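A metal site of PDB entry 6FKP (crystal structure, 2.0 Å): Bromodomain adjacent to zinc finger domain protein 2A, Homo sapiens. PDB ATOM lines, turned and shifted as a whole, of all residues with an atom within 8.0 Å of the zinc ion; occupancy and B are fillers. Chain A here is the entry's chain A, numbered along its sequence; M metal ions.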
ATOM      1  N   LEU A  10     -10.919 -26.668  -3.335  1.00  0.00           N
ATOM      2  CA  LEU A  10     -11.895 -25.575  -3.167  1.00  0.00           C
ATOM      3  C   LEU A  10     -13.303 -26.033  -2.786  1.00  0.00           C
ATOM      4  O   LEU A  10     -14.035 -25.290  -2.128  1.00  0.00           O
ATOM      5  CB  LEU A  10     -11.998 -24.747  -4.453  1.00  0.00           C
ATOM      6  CG  LEU A  10     -10.871 -23.772  -4.753  1.00  0.00           C
ATOM      7  CD1 LEU A  10     -10.944 -23.329  -6.210  1.00  0.00           C
ATOM      8  CD2 LEU A  10     -10.942 -22.577  -3.821  1.00  0.00           C
ATOM      9  N   LEU A  23      -4.251 -28.892  -9.718  1.00  0.00           N
ATOM     10  CA  LEU A  23      -3.699 -27.579  -9.357  1.00  0.00           C
ATOM     11  C   LEU A  23      -3.996 -26.529 -10.418  1.00  0.00           C
ATOM     12  O   LEU A  23      -3.861 -26.791 -11.624  1.00  0.00           O
ATOM     13  CB  LEU A  23      -2.185 -27.682  -9.165  1.00  0.00           C
ATOM     14  CG  LEU A  23      -1.692 -28.663  -8.102  1.00  0.00           C
ATOM     15  CD1 LEU A  23      -0.166 -28.633  -8.036  1.00  0.00           C
ATOM     16  CD2 LEU A  23      -2.285 -28.353  -6.734  1.00  0.00           C
ATOM     17  N   CYS A  24      -4.402 -25.346  -9.973  1.00  0.00           N
ATOM     18  CA  CYS A  24      -4.657 -24.230 -10.880  1.00  0.00           C
ATOM     19  C   CYS A  24      -3.344 -23.693 -11.459  1.00  0.00           C
ATOM     20  O   CYS A  24      -2.365 -23.539 -10.726  1.00  0.00           O
ATOM     21  CB  CYS A  24      -5.409 -23.112 -10.161  1.00  0.00           C
ATOM     22  SG  CYS A  24      -5.791 -21.714 -11.232  1.00  0.00           S
ATOM     23  N   ASP A  25      -3.331 -23.436 -12.766  1.00  0.00           N
ATOM     24  CA  ASP A  25      -2.156 -22.849 -13.429  1.00  0.00           C
ATOM     25  C   ASP A  25      -2.062 -21.321 -13.297  1.00  0.00           C
ATOM     26  O   ASP A  25      -1.072 -20.735 -13.728  1.00  0.00           O
ATOM     27  CB  ASP A  25      -2.135 -23.247 -14.915  1.00  0.00           C
ATOM     28  CG  ASP A  25      -1.900 -24.736 -15.098  1.00  0.00           C
ATOM     29  OD1 ASP A  25      -0.778 -25.184 -14.815  1.00  0.00           O
ATOM     30  OD2 ASP A  25      -2.842 -25.445 -15.507  1.00  0.00           O
ATOM     31  N   GLY A  26      -3.089 -20.692 -12.712  1.00  0.00           N
ATOM     32  CA  GLY A  26      -3.095 -19.254 -12.457  1.00  0.00           C
ATOM     33  C   GLY A  26      -2.873 -18.829 -11.013  1.00  0.00           C
ATOM     34  O   GLY A  26      -2.651 -17.637 -10.751  1.00  0.00           O
ATOM     35  N   CYS A  27      -2.950 -19.774 -10.065  1.00  0.00           N
ATOM     36  CA  CYS A  27      -2.816 -19.459  -8.628  1.00  0.00           C
ATOM     37  C   CYS A  27      -2.457 -20.716  -7.813  1.00  0.00           C
ATOM     38  O   CYS A  27      -2.164 -21.765  -8.390  1.00  0.00           O
ATOM     39  CB  CYS A  27      -4.112 -18.811  -8.113  1.00  0.00           C
ATOM     40  SG  CYS A  27      -5.496 -19.942  -7.839  1.00  0.00           S
ATOM     41  N   ASP A  28      -2.483 -20.611  -6.478  1.00  0.00           N
ATOM     42  CA  ASP A  28      -2.141 -21.741  -5.597  1.00  0.00           C
ATOM     43  C   ASP A  28      -3.310 -22.694  -5.264  1.00  0.00           C
ATOM     44  O   ASP A  28      -3.121 -23.641  -4.496  1.00  0.00           O
ATOM     45  CB  ASP A  28      -1.544 -21.208  -4.289  1.00  0.00           C
ATOM     46  N   ARG A  29      -4.485 -22.465  -5.862  1.00  0.00           N
ATOM     47  CA  ARG A  29      -5.701 -23.195  -5.466  1.00  0.00           C
ATOM     48  C   ARG A  29      -5.785 -24.543  -6.165  1.00  0.00           C
ATOM     49  O   ARG A  29      -5.107 -24.769  -7.176  1.00  0.00           O
ATOM     50  CB  ARG A  29      -6.955 -22.378  -5.750  1.00  0.00           C
ATOM     51  CG  ARG A  29      -7.166 -21.208  -4.809  1.00  0.00           C
ATOM     52  CD  ARG A  29      -8.172 -20.213  -5.352  1.00  0.00           C
ATOM     53  NE  ARG A  29      -8.315 -19.036  -4.495  1.00  0.00           N
ATOM     54  CZ  ARG A  29      -7.681 -17.876  -4.646  1.00  0.00           C
ATOM     55  NH1 ARG A  29      -6.835 -17.658  -5.651  1.00  0.00           N
ATOM     56  NH2 ARG A  29      -7.906 -16.890  -3.775  1.00  0.00           N
ATOM     57  N   GLY A  30      -6.620 -25.412  -5.623  1.00  0.00           N
ATOM     58  CA  GLY A  30      -6.768 -26.775  -6.126  1.00  0.00           C
ATOM     59  C   GLY A  30      -8.190 -27.273  -6.111  1.00  0.00           C
ATOM     60  O   GLY A  30      -9.078 -26.665  -5.501  1.00  0.00           O
ATOM     61  N   TRP A  48      -5.435 -25.737 -16.667  1.00  0.00           N
ATOM     62  CA  TRP A  48      -6.713 -25.621 -15.963  1.00  0.00           C
ATOM     63  C   TRP A  48      -6.696 -24.386 -15.054  1.00  0.00           C
ATOM     64  O   TRP A  48      -5.728 -24.160 -14.319  1.00  0.00           O
ATOM     65  CB  TRP A  48      -7.025 -26.879 -15.135  1.00  0.00           C
ATOM     66  CG  TRP A  48      -8.296 -26.745 -14.364  1.00  0.00           C
ATOM     67  CD1 TRP A  48      -9.564 -26.801 -14.862  1.00  0.00           C
ATOM     68  CD2 TRP A  48      -8.427 -26.470 -12.967  1.00  0.00           C
ATOM     69  NE1 TRP A  48     -10.477 -26.595 -13.862  1.00  0.00           N
ATOM     70  CE2 TRP A  48      -9.814 -26.388 -12.678  1.00  0.00           C
ATOM     71  CE3 TRP A  48      -7.515 -26.291 -11.918  1.00  0.00           C
ATOM     72  CZ2 TRP A  48     -10.299 -26.141 -11.395  1.00  0.00           C
ATOM     73  CZ3 TRP A  48      -7.993 -26.039 -10.641  1.00  0.00           C
ATOM     74  CH2 TRP A  48      -9.380 -25.964 -10.389  1.00  0.00           C
ATOM     75  N   PHE A  49      -7.768 -23.601 -15.127  1.00  0.00           N
ATOM     76  CA  PHE A  49      -7.929 -22.400 -14.306  1.00  0.00           C
ATOM     77  C   PHE A  49      -9.110 -22.556 -13.366  1.00  0.00           C
ATOM     78  O   PHE A  49     -10.207 -22.951 -13.787  1.00  0.00           O
ATOM     79  CB  PHE A  49      -8.083 -21.158 -15.182  1.00  0.00           C
ATOM     80  CG  PHE A  49      -6.815 -20.785 -15.901  1.00  0.00           C
ATOM     81  CD1 PHE A  49      -5.751 -20.216 -15.209  1.00  0.00           C
ATOM     82  CD2 PHE A  49      -6.669 -21.038 -17.267  1.00  0.00           C
ATOM     83  CE1 PHE A  49      -4.566 -19.899 -15.861  1.00  0.00           C
ATOM     84  CE2 PHE A  49      -5.484 -20.721 -17.919  1.00  0.00           C
ATOM     85  CZ  PHE A  49      -4.439 -20.147 -17.212  1.00  0.00           C
ATOM     86  N   CYS A  50      -8.876 -22.265 -12.095  1.00  0.00           N
ATOM     87  CA  CYS A  50      -9.939 -22.266 -11.086  1.00  0.00           C
ATOM     88  C   CYS A  50     -10.898 -21.091 -11.315  1.00  0.00           C
ATOM     89  O   CYS A  50     -10.625 -20.177 -12.102  1.00  0.00           O
ATOM     90  CB  CYS A  50      -9.361 -22.167  -9.678  1.00  0.00           C
ATOM     91  SG  CYS A  50      -8.854 -20.499  -9.214  1.00  0.00           S
ATOM     92  N   THR A  51     -12.015 -21.105 -10.585  1.00  0.00           N
ATOM     93  CA  THR A  51     -13.054 -20.089 -10.730  1.00  0.00           C
ATOM     94  C   THR A  51     -12.632 -18.676 -10.315  1.00  0.00           C
ATOM     95  O   THR A  51     -13.130 -17.694 -10.880  1.00  0.00           O
ATOM     96  CB  THR A  51     -14.327 -20.505  -9.964  1.00  0.00           C
ATOM     97  OG1 THR A  51     -13.963 -21.042  -8.688  1.00  0.00           O
ATOM     98  CG2 THR A  51     -15.061 -21.575 -10.754  1.00  0.00           C
ATOM     99  N   VAL A  52     -11.702 -18.559  -9.368  1.00  0.00           N
ATOM    100  CA  VAL A  52     -11.175 -17.255  -8.976  1.00  0.00           C
ATOM    101  C   VAL A  52     -10.356 -16.662 -10.138  1.00  0.00           C
ATOM    102  O   VAL A  52     -10.532 -15.497 -10.474  1.00  0.00           O
ATOM    103  CB  VAL A  52     -10.328 -17.318  -7.687  1.00  0.00           C
ATOM    104  CG1 VAL A  52      -9.744 -15.958  -7.341  1.00  0.00           C
ATOM    105  CG2 VAL A  52     -11.174 -17.844  -6.528  1.00  0.00           C
ATOM    106  N   CYS A  53      -9.495 -17.474 -10.749  1.00  0.00           N
ATOM    107  CA  CYS A  53      -8.753 -17.044 -11.940  1.00  0.00           C
ATOM    108  C   CYS A  53      -9.629 -16.745 -13.154  1.00  0.00           C
ATOM    109  O   CYS A  53      -9.386 -15.766 -13.866  1.00  0.00           O
ATOM    110  CB  CYS A  53      -7.675 -18.071 -12.294  1.00  0.00           C
ATOM    111  SG  CYS A  53      -6.347 -18.088 -11.066  1.00  0.00           S
ATOM    112  N   LEU A  54     -10.676 -17.545 -13.380  1.00  0.00           N
ATOM    113  CA  LEU A  54     -11.644 -17.245 -14.451  1.00  0.00           C
ATOM    114  C   LEU A  54     -12.293 -15.880 -14.265  1.00  0.00           C
ATOM    115  O   LEU A  54     -12.541 -15.163 -15.248  1.00  0.00           O
ATOM    116  CB  LEU A  54     -12.733 -18.317 -14.546  1.00  0.00           C
ATOM    117  CG  LEU A  54     -12.332 -19.703 -15.031  1.00  0.00           C
ATOM    118  CD1 LEU A  54     -13.560 -20.608 -15.006  1.00  0.00           C
ATOM    119  CD2 LEU A  54     -11.726 -19.659 -16.429  1.00  0.00           C
ATOM    120  N   GLN A  56     -10.861 -13.260 -13.124  1.00  0.00           N
ATOM    121  CA  GLN A  56      -9.886 -12.205 -13.489  1.00  0.00           C
ATOM    122  C   GLN A  56      -9.719 -12.004 -15.004  1.00  0.00           C
ATOM    123  O   GLN A  56      -9.144 -10.998 -15.433  1.00  0.00           O
ATOM    124  CB  GLN A  56      -8.510 -12.478 -12.862  1.00  0.00           C
ATOM    125  CG  GLN A  56      -8.516 -12.886 -11.387  1.00  0.00           C
ATOM    126  CD  GLN A  56      -9.474 -12.075 -10.526  1.00  0.00           C
ATOM    127  OE1 GLN A  56      -9.381 -10.850 -10.464  1.00  0.00           O
ATOM    128  NE2 GLN A  56     -10.409 -12.764  -9.861  1.00  0.00           N
HETATM  129 ZN    ZN M   1      -6.645 -20.057  -9.849  1.00  0.00          ZN
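SG of Cys 27 sits close to N of Arg 29, at 3.4 Å. SG of Cys 24 sits close to N of Gly 26 (3.2 Å). The backbone NH (N) of Cys 24 sits at hydrogen-bond distance from the backbone carbonyl oxygen (O) of Arg 29, 2.9 Å away. The backbone carbonyl oxygen (O) of Gly 26 sits close to the side-chain sulfur (SG) of Cys 53. The backbone NH (N) of Val 52 lies close to the side-chain sulfur (SG) of Cys 50, 3.4 Å away.
Four residues have an atom within 4 Å of the zinc ion: Cys 24, Cys 27, Cys 50 and Cys 53. The nearest printed residue that does not touch the zinc ion is Gly 26 (4.1 Å).
The zinc ion is bound by SG of Cys 27 (2.3 Å), SG of Cys 24 (2.3 Å), SG of Cys 53 (2.3 Å) and SG of Cys 50 (2.3 Å).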
